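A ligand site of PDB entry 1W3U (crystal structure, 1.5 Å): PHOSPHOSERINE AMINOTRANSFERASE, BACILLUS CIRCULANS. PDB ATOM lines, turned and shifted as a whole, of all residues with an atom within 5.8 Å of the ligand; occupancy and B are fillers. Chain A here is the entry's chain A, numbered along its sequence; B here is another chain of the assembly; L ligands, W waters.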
ATOM      1  N   ALA A  10     -34.069   0.330  -3.161  1.00  0.00           N
ATOM      2  CA  ALA A  10     -32.628   0.242  -3.270  1.00  0.00           C
ATOM      3  C   ALA A  10     -32.077  -1.133  -2.975  1.00  0.00           C
ATOM      4  O   ALA A  10     -30.875  -1.311  -3.099  1.00  0.00           O
ATOM      5  CB  ALA A  10     -32.003   1.264  -2.295  1.00  0.00           C
ATOM      6  N   GLY A  75     -25.868 -15.615   2.831  1.00  0.00           N
ATOM      7  CA  GLY A  75     -25.452 -14.710   3.902  1.00  0.00           C
ATOM      8  C   GLY A  75     -25.342 -13.249   3.530  1.00  0.00           C
ATOM      9  O   GLY A  75     -25.022 -12.389   4.364  1.00  0.00           O
ATOM     10  N   GLY A  76     -25.582 -12.900   2.269  1.00  0.00           N
ATOM     11  CA  GLY A  76     -25.508 -11.531   1.797  1.00  0.00           C
ATOM     12  C   GLY A  76     -24.095 -11.010   1.663  1.00  0.00           C
ATOM     13  O   GLY A  76     -23.094 -11.665   2.028  1.00  0.00           O
ATOM     14  N   ALA A  77     -23.992  -9.793   1.155  1.00  0.00           N
ATOM     15  CA  ALA A  77     -22.675  -9.159   1.096  1.00  0.00           C
ATOM     16  C   ALA A  77     -22.146  -8.975   2.511  1.00  0.00           C
ATOM     17  O   ALA A  77     -20.923  -9.024   2.738  1.00  0.00           O
ATOM     18  CB  ALA A  77     -22.711  -7.816   0.389  1.00  0.00           C
ATOM     19  N   SER A  78     -23.048  -8.777   3.478  1.00  0.00           N
ATOM     20  CA  SER A  78     -22.550  -8.546   4.818  1.00  0.00           C
ATOM     21  C   SER A  78     -21.741  -9.746   5.316  1.00  0.00           C
ATOM     22  O   SER A  78     -20.802  -9.561   6.076  1.00  0.00           O
ATOM     23  CB  SER A  78     -23.761  -8.348   5.714  1.00  0.00           C
ATOM     24  OG  SER A  78     -24.425  -7.144   5.389  1.00  0.00           O
ATOM     25  N   THR A  79     -22.127 -10.966   4.906  1.00  0.00           N
ATOM     26  CA  THR A  79     -21.324 -12.118   5.360  1.00  0.00           C
ATOM     27  C   THR A  79     -19.971 -12.110   4.655  1.00  0.00           C
ATOM     28  O   THR A  79     -18.979 -12.519   5.258  1.00  0.00           O
ATOM     29  CB  THR A  79     -22.107 -13.391   5.127  1.00  0.00           C
ATOM     30  OG1 THR A  79     -23.235 -13.444   6.017  1.00  0.00           O
ATOM     31  CG2 THR A  79     -21.247 -14.648   5.376  1.00  0.00           C
ATOM     32  N   PHE A  81     -18.261  -9.559   4.138  1.00  0.00           N
ATOM     33  CA  PHE A  81     -17.410  -8.633   4.884  1.00  0.00           C
ATOM     34  C   PHE A  81     -16.556  -9.381   5.907  1.00  0.00           C
ATOM     35  O   PHE A  81     -15.440  -8.969   6.166  1.00  0.00           O
ATOM     36  CB  PHE A  81     -18.228  -7.591   5.641  1.00  0.00           C
ATOM     37  CG  PHE A  81     -18.986  -6.589   4.785  1.00  0.00           C
ATOM     38  CD1 PHE A  81     -18.649  -6.323   3.476  1.00  0.00           C
ATOM     39  CD2 PHE A  81     -20.046  -5.929   5.405  1.00  0.00           C
ATOM     40  CE1 PHE A  81     -19.396  -5.378   2.755  1.00  0.00           C
ATOM     41  CE2 PHE A  81     -20.802  -5.014   4.679  1.00  0.00           C
ATOM     42  CZ  PHE A  81     -20.452  -4.749   3.354  1.00  0.00           C
ATOM     43  N   TRP A 103     -20.933   1.686   2.997  1.00  0.00           N
ATOM     44  CA  TRP A 103     -20.681   0.242   2.877  1.00  0.00           C
ATOM     45  C   TRP A 103     -19.199  -0.040   3.032  1.00  0.00           C
ATOM     46  O   TRP A 103     -18.855  -1.098   3.575  1.00  0.00           O
ATOM     47  CB  TRP A 103     -21.270  -0.259   1.563  1.00  0.00           C
ATOM     48  CG  TRP A 103     -22.780  -0.370   1.700  1.00  0.00           C
ATOM     49  CD1 TRP A 103     -23.733   0.316   1.006  1.00  0.00           C
ATOM     50  CD2 TRP A 103     -23.455  -1.225   2.606  1.00  0.00           C
ATOM     51  NE1 TRP A 103     -24.975  -0.079   1.442  1.00  0.00           N
ATOM     52  CE2 TRP A 103     -24.839  -1.034   2.440  1.00  0.00           C
ATOM     53  CE3 TRP A 103     -23.004  -2.154   3.552  1.00  0.00           C
ATOM     54  CZ2 TRP A 103     -25.794  -1.723   3.165  1.00  0.00           C
ATOM     55  CZ3 TRP A 103     -23.968  -2.832   4.271  1.00  0.00           C
ATOM     56  CH2 TRP A 103     -25.340  -2.632   4.089  1.00  0.00           C
ATOM     57  N   THR A 149     -15.263  -0.426  -2.584  1.00  0.00           N
ATOM     58  CA  THR A 149     -16.688  -0.577  -2.822  1.00  0.00           C
ATOM     59  C   THR A 149     -16.979   0.091  -4.155  1.00  0.00           C
ATOM     60  O   THR A 149     -16.729   1.297  -4.276  1.00  0.00           O
ATOM     61  CB  THR A 149     -17.423   0.086  -1.653  1.00  0.00           C
ATOM     62  OG1 THR A 149     -16.930  -0.425  -0.409  1.00  0.00           O
ATOM     63  CG2 THR A 149     -18.920  -0.192  -1.778  1.00  0.00           C
ATOM     64  N   ASN A 151     -19.568   0.887  -5.921  1.00  0.00           N
ATOM     65  CA  ASN A 151     -20.723   1.782  -5.907  1.00  0.00           C
ATOM     66  C   ASN A 151     -21.236   1.939  -4.492  1.00  0.00           C
ATOM     67  O   ASN A 151     -21.673   0.976  -3.880  1.00  0.00           O
ATOM     68  CB  ASN A 151     -21.786   1.241  -6.877  1.00  0.00           C
ATOM     69  CG  ASN A 151     -22.934   2.222  -7.023  1.00  0.00           C
ATOM     70  OD1 ASN A 151     -22.815   3.193  -7.777  1.00  0.00           O
ATOM     71  ND2 ASN A 151     -24.030   1.984  -6.304  1.00  0.00           N
ATOM     72  N   GLU A 152     -21.151   3.163  -3.934  1.00  0.00           N
ATOM     73  CA  GLU A 152     -21.596   3.350  -2.543  1.00  0.00           C
ATOM     74  C   GLU A 152     -23.088   3.664  -2.619  1.00  0.00           C
ATOM     75  O   GLU A 152     -23.520   4.777  -2.966  1.00  0.00           O
ATOM     76  CB  GLU A 152     -20.750   4.443  -1.893  1.00  0.00           C
ATOM     77  CG  GLU A 152     -19.363   3.970  -1.427  1.00  0.00           C
ATOM     78  CD  GLU A 152     -19.405   3.192  -0.118  1.00  0.00           C
ATOM     79  OE1 GLU A 152     -20.515   2.808   0.343  1.00  0.00           O
ATOM     80  OE2 GLU A 152     -18.353   2.964   0.487  1.00  0.00           O
ATOM     81  N   THR A 153     -23.824   2.624  -2.307  1.00  0.00           N
ATOM     82  CA  THR A 153     -25.246   2.602  -2.584  1.00  0.00           C
ATOM     83  C   THR A 153     -26.009   3.684  -1.850  1.00  0.00           C
ATOM     84  O   THR A 153     -27.033   4.176  -2.315  1.00  0.00           O
ATOM     85  CB  THR A 153     -25.799   1.267  -2.062  1.00  0.00           C
ATOM     86  OG1 THR A 153     -24.833   0.293  -2.469  1.00  0.00           O
ATOM     87  CG2 THR A 153     -27.118   0.925  -2.716  1.00  0.00           C
ATOM     88  N   ASP A 173     -16.501  -4.825  -3.478  1.00  0.00           N
ATOM     89  CA  ASP A 173     -17.915  -4.992  -3.167  1.00  0.00           C
ATOM     90  C   ASP A 173     -18.726  -4.307  -4.280  1.00  0.00           C
ATOM     91  O   ASP A 173     -18.837  -3.096  -4.273  1.00  0.00           O
ATOM     92  CB  ASP A 173     -18.224  -4.397  -1.798  1.00  0.00           C
ATOM     93  CG  ASP A 173     -19.677  -4.461  -1.406  1.00  0.00           C
ATOM     94  OD1 ASP A 173     -20.486  -4.959  -2.233  1.00  0.00           O
ATOM     95  OD2 ASP A 173     -19.997  -4.001  -0.267  1.00  0.00           O
ATOM     96  N   MET A 174     -19.259  -5.137  -5.165  1.00  0.00           N
ATOM     97  CA  MET A 174     -20.007  -4.583  -6.290  1.00  0.00           C
ATOM     98  C   MET A 174     -21.509  -4.834  -6.144  1.00  0.00           C
ATOM     99  O   MET A 174     -22.217  -4.936  -7.144  1.00  0.00           O
ATOM    100  CB  MET A 174     -19.530  -5.178  -7.633  1.00  0.00           C
ATOM    101  CG  MET A 174     -18.048  -4.870  -7.871  1.00  0.00           C
ATOM    102  SD  MET A 174     -17.660  -5.404  -9.559  1.00  0.00           S
ATOM    103  CE  MET A 174     -16.009  -4.714  -9.730  1.00  0.00           C
ATOM    104  N   SER A 175     -21.932  -4.931  -4.892  1.00  0.00           N
ATOM    105  CA  SER A 175     -23.339  -5.229  -4.622  1.00  0.00           C
ATOM    106  C   SER A 175     -24.322  -4.395  -5.443  1.00  0.00           C
ATOM    107  O   SER A 175     -25.247  -4.966  -6.017  1.00  0.00           O
ATOM    108  CB  SER A 175     -23.612  -5.040  -3.126  1.00  0.00           C
ATOM    109  OG  SER A 175     -22.985  -6.053  -2.344  1.00  0.00           O
ATOM    110  N   SER A 176     -24.061  -3.098  -5.532  1.00  0.00           N
ATOM    111  CA  SER A 176     -25.104  -2.260  -6.160  1.00  0.00           C
ATOM    112  C   SER A 176     -24.753  -1.867  -7.588  1.00  0.00           C
ATOM    113  O   SER A 176     -25.482  -1.069  -8.215  1.00  0.00           O
ATOM    114  CB  SER A 176     -25.386  -1.055  -5.252  1.00  0.00           C
ATOM    115  OG  SER A 176     -24.184  -0.391  -4.897  1.00  0.00           O
ATOM    116  N   TYR A 192     -17.689  -9.338  -5.311  1.00  0.00           N
ATOM    117  CA  TYR A 192     -18.895  -9.950  -4.754  1.00  0.00           C
ATOM    118  C   TYR A 192     -20.091  -9.006  -4.785  1.00  0.00           C
ATOM    119  O   TYR A 192     -19.882  -7.789  -4.886  1.00  0.00           O
ATOM    120  CB  TYR A 192     -18.688 -10.315  -3.317  1.00  0.00           C
ATOM    121  CG  TYR A 192     -18.319  -9.300  -2.285  1.00  0.00           C
ATOM    122  CD1 TYR A 192     -17.071  -8.704  -2.270  1.00  0.00           C
ATOM    123  CD2 TYR A 192     -19.226  -8.922  -1.314  1.00  0.00           C
ATOM    124  CE1 TYR A 192     -16.722  -7.771  -1.327  1.00  0.00           C
ATOM    125  CE2 TYR A 192     -18.887  -7.999  -0.341  1.00  0.00           C
ATOM    126  CZ  TYR A 192     -17.641  -7.413  -0.340  1.00  0.00           C
ATOM    127  OH  TYR A 192     -17.270  -6.490   0.608  1.00  0.00           O
ATOM    128  N   GLY A 194     -24.372  -8.999  -3.153  1.00  0.00           N
ATOM    129  CA  GLY A 194     -25.676  -9.607  -2.846  1.00  0.00           C
ATOM    130  C   GLY A 194     -26.481  -9.466  -4.154  1.00  0.00           C
ATOM    131  O   GLY A 194     -26.455  -8.452  -4.803  1.00  0.00           O
ATOM    132  N   GLN A 196     -29.627  -9.168  -4.682  1.00  0.00           N
ATOM    133  CA  GLN A 196     -30.875  -8.451  -4.608  1.00  0.00           C
ATOM    134  C   GLN A 196     -30.814  -7.013  -5.080  1.00  0.00           C
ATOM    135  O   GLN A 196     -31.900  -6.389  -5.119  1.00  0.00           O
ATOM    136  CB  GLN A 196     -31.406  -8.473  -3.165  1.00  0.00           C
ATOM    137  CG  GLN A 196     -30.610  -7.621  -2.181  1.00  0.00           C
ATOM    138  CD  GLN A 196     -29.463  -8.379  -1.526  1.00  0.00           C
ATOM    139  OE1 GLN A 196     -29.050  -9.461  -1.948  1.00  0.00           O
ATOM    140  NE2 GLN A 196     -28.916  -7.804  -0.472  1.00  0.00           N
ATOM    141  N   LYS A 197     -29.640  -6.465  -5.396  1.00  0.00           N
ATOM    142  CA  LYS A 197     -29.703  -5.119  -5.985  1.00  0.00           C
ATOM    143  C   LYS A 197     -29.803  -5.147  -7.505  1.00  0.00           C
ATOM    144  O   LYS A 197     -30.751  -4.578  -8.104  1.00  0.00           O
ATOM    145  CB  LYS A 197     -28.478  -4.331  -5.514  1.00  0.00           C
ATOM    146  CG  LYS A 197     -28.732  -3.656  -4.168  1.00  0.00           C
ATOM    147  CD  LYS A 197     -28.223  -4.439  -3.005  1.00  0.00           C
ATOM    148  CE  LYS A 197     -28.675  -3.755  -1.697  1.00  0.00           C
ATOM    149  NZ  LYS A 197     -27.425  -3.164  -1.089  1.00  0.00           N
ATOM    150  N   THR A 205     -25.645 -14.545  -2.722  1.00  0.00           N
ATOM    151  CA  THR A 205     -24.536 -13.675  -2.959  1.00  0.00           C
ATOM    152  C   THR A 205     -23.669 -14.286  -4.054  1.00  0.00           C
ATOM    153  O   THR A 205     -23.248 -15.435  -3.940  1.00  0.00           O
ATOM    154  CB  THR A 205     -23.702 -13.466  -1.664  1.00  0.00           C
ATOM    155  OG1 THR A 205     -24.667 -13.018  -0.701  1.00  0.00           O
ATOM    156  CG2 THR A 205     -22.623 -12.423  -1.815  1.00  0.00           C
ATOM    157  N   TYR A 339     -31.176   0.646 -10.873  1.00  0.00           N
ATOM    158  CA  TYR A 339     -30.569  -0.598 -11.332  1.00  0.00           C
ATOM    159  C   TYR A 339     -31.040  -1.042 -12.720  1.00  0.00           C
ATOM    160  O   TYR A 339     -32.021  -0.480 -13.193  1.00  0.00           O
ATOM    161  CB  TYR A 339     -30.966  -1.662 -10.309  1.00  0.00           C
ATOM    162  CG  TYR A 339     -30.520  -1.297  -8.887  1.00  0.00           C
ATOM    163  CD1 TYR A 339     -29.189  -0.995  -8.612  1.00  0.00           C
ATOM    164  CD2 TYR A 339     -31.423  -1.268  -7.865  1.00  0.00           C
ATOM    165  CE1 TYR A 339     -28.805  -0.674  -7.323  1.00  0.00           C
ATOM    166  CE2 TYR A 339     -31.043  -0.937  -6.555  1.00  0.00           C
ATOM    167  CZ  TYR A 339     -29.727  -0.645  -6.291  1.00  0.00           C
ATOM    168  OH  TYR A 339     -29.323  -0.314  -5.013  1.00  0.00           O
ATOM    169  N   GLN B  74     -29.493 -17.086   7.052  1.00  0.00           N
ATOM    170  CA  GLN B  74     -29.045 -17.739   5.815  1.00  0.00           C
ATOM    171  C   GLN B  74     -27.919 -18.736   6.121  1.00  0.00           C
ATOM    172  O   GLN B  74     -27.377 -18.790   7.227  1.00  0.00           O
ATOM    173  CB  GLN B  74     -28.549 -16.675   4.843  1.00  0.00           C
ATOM    174  CG  GLN B  74     -29.655 -15.722   4.378  1.00  0.00           C
ATOM    175  CD  GLN B  74     -29.112 -14.719   3.380  1.00  0.00           C
ATOM    176  OE1 GLN B  74     -28.585 -15.187   2.349  1.00  0.00           O
ATOM    177  NE2 GLN B  74     -29.231 -13.402   3.642  1.00  0.00           N
ATOM    178  N   MET B 224     -22.448 -11.058  11.526  1.00  0.00           N
ATOM    179  CA  MET B 224     -23.463 -11.979  10.981  1.00  0.00           C
ATOM    180  C   MET B 224     -23.496 -13.363  11.597  1.00  0.00           C
ATOM    181  O   MET B 224     -24.377 -14.199  11.252  1.00  0.00           O
ATOM    182  CB  MET B 224     -23.184 -12.117   9.475  1.00  0.00           C
ATOM    183  CG  MET B 224     -23.528 -10.804   8.762  1.00  0.00           C
ATOM    184  SD  MET B 224     -25.277 -10.366   8.789  1.00  0.00           S
ATOM    185  CE  MET B 224     -25.943 -11.699   7.792  1.00  0.00           C
ATOM    186  N   ASN B 238     -29.385  -7.288   8.067  1.00  0.00           N
ATOM    187  CA  ASN B 238     -29.041  -7.155   6.653  1.00  0.00           C
ATOM    188  C   ASN B 238     -30.234  -7.671   5.836  1.00  0.00           C
ATOM    189  O   ASN B 238     -31.307  -7.973   6.411  1.00  0.00           O
ATOM    190  CB  ASN B 238     -27.745  -7.879   6.302  1.00  0.00           C
ATOM    191  CG  ASN B 238     -27.885  -9.364   6.086  1.00  0.00           C
ATOM    192  OD1 ASN B 238     -28.670 -10.015   6.751  1.00  0.00           O
ATOM    193  ND2 ASN B 238     -27.063  -9.881   5.130  1.00  0.00           N
ATOM    194  N   THR B 239     -30.013  -7.785   4.524  1.00  0.00           N
ATOM    195  CA  THR B 239     -31.161  -8.221   3.713  1.00  0.00           C
ATOM    196  C   THR B 239     -31.484  -9.685   3.936  1.00  0.00           C
ATOM    197  O   THR B 239     -30.590 -10.503   3.734  1.00  0.00           O
ATOM    198  CB  THR B 239     -30.907  -8.009   2.217  1.00  0.00           C
ATOM    199  OG1 THR B 239     -30.440  -6.676   2.006  1.00  0.00           O
ATOM    200  CG2 THR B 239     -32.242  -8.093   1.480  1.00  0.00           C
HETATM  201  N1  LIG L   1     -22.601  -3.630   0.193  1.00  0.00           N
HETATM  202  C1  LIG L   1     -23.271  -2.829  -0.678  1.00  0.00           C
HETATM  203  C2  LIG L   1     -22.457  -1.925  -1.618  1.00  0.00           C
HETATM  204  C3  LIG L   1     -24.650  -2.844  -0.697  1.00  0.00           C
HETATM  205  O1  LIG L   1     -25.280  -2.024  -1.588  1.00  0.00           O
HETATM  206  C4  LIG L   1     -25.345  -3.660   0.167  1.00  0.00           C
HETATM  207  C5  LIG L   1     -26.888  -3.745   0.165  1.00  0.00           C
HETATM  208  C6  LIG L   1     -24.646  -4.471   1.049  1.00  0.00           C
HETATM  209  C7  LIG L   1     -23.284  -4.446   1.041  1.00  0.00           C
HETATM  210  C8  LIG L   1     -25.356  -5.404   2.018  1.00  0.00           C
HETATM  211  O2  LIG L   1     -25.920  -6.548   1.395  1.00  0.00           O
HETATM  212  P1  LIG L   1     -26.679  -7.624   2.267  1.00  0.00           P
HETATM  213  O3  LIG L   1     -27.019  -8.766   1.349  1.00  0.00           O
HETATM  214  O4  LIG L   1     -27.919  -6.965   2.826  1.00  0.00           O
HETATM  215  O5  LIG L   1     -25.740  -8.060   3.371  1.00  0.00           O
HETATM  216  O   HOH W   1     -21.485  -1.791  -4.866  1.00  0.00           O
HETATM  217  O   HOH W   2     -28.120  -4.763   4.434  1.00  0.00           O
HETATM  218  O   HOH W   3     -28.530 -10.791   2.154  1.00  0.00           O
HETATM  219  O   HOH W   4     -25.499  -6.899  -1.367  1.00  0.00           O
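N1 of the ligand sits at hydrogen-bond distance from OD2 of Asp 173 (2.7 Å).
OG of Ser 78 is in hydrogen-bond range of O5 of the ligand, at 2.6 Å.
NZ of Lys 197 is bonded to C5 of the ligand, 1.5 Å away.
The side-chain amide nitrogen (NE2) of Gln 196 sits at hydrogen-bond distance from an oxygen (O3) of the ligand, at 2.8 Å.
OG1 of Thr 239 of chain B sits at hydrogen-bond distance from O4 of the ligand (2.7 Å).
The side-chain amide nitrogen of Asn 238 of chain B sits at hydrogen-bond distance from an oxygen (O5) of the ligand, 2.9 Å away.
N of Ala 77 lies within hydrogen-bond range of O3 of the ligand, 3.2 Å away.
N of Ser 78 sits at hydrogen-bond distance from O5 of the ligand (2.8 Å).
O4 of the ligand is in hydrogen-bond range of N of Thr 239 of chain B, at 2.8 Å.
OG1 of Thr 153 is in hydrogen-bond range of O1 of the ligand.
The backbone carbonyl oxygen of Thr 239 of chain B lies within hydrogen-bond range of the side-chain amide nitrogen of Gln 74 of chain B (3.2 Å).
OG of Ser 176 sits at hydrogen-bond distance from OG1 of Thr 153.
The side-chain hydroxyl of Thr 205 sits close to the backbone NH of Gly 76 (3.1 Å).
The side-chain hydroxyl (OG) of Ser 176 is in hydrogen-bond range of the side-chain amide nitrogen (ND2) of Asn 151 (2.8 Å).
ND2 of Asn 238 of chain B sits at hydrogen-bond distance from O of Gly 75.
The side-chain hydroxyl (OG1) of Thr 239 of chain B is in hydrogen-bond range of the side-chain amide nitrogen (NE2) of Gln 196, 3.1 Å away.
The backbone NH of Gly 194 is in hydrogen-bond range of the side-chain hydroxyl of Ser 175, 3.4 Å away.
N of Trp 103 sits at hydrogen-bond distance from OE1 of Glu 152 (2.9 Å).
Gly 76 touches the ligand (CA to O3, 3.2 Å).
Phe 81 touches the ligand.
Trp 103 touches the ligand.
Thr 149 touches the ligand.
Asn 151 touches the ligand (O to C2, 3.8 Å).
CB of Ser 175 touches C1 of the ligand, 3.3 Å away.
Ser 176 touches the ligand (CB to O1, 3.8 Å).
Hydrophobic or aromatic side chains that line the ligand: Ala 77, Phe 81 and Trp 103.
Of the 26 residues printed, 15 come within 4 Å of the ligand.
Water W3 lies within hydrogen-bond range of the backbone carbonyl oxygen of Thr 239 of chain B (2.6 Å), an oxygen (O3) of the ligand (2.7 Å), the side-chain amide nitrogen of Gln 74 of chain B (3.1 Å) and the side-chain amide nitrogen of Asn 238 of chain B (3.4 Å).
Water W4 lies within hydrogen-bond range of O2 of the ligand, OG of Ser 175 and N of Gly 194.
Water W1 lies within hydrogen-bond range of O of Asn 151 (2.9 Å), N of Ser 176 (3.0 Å), O of Asp 173 (3.0 Å) and N of Ser 175 (3.2 Å).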
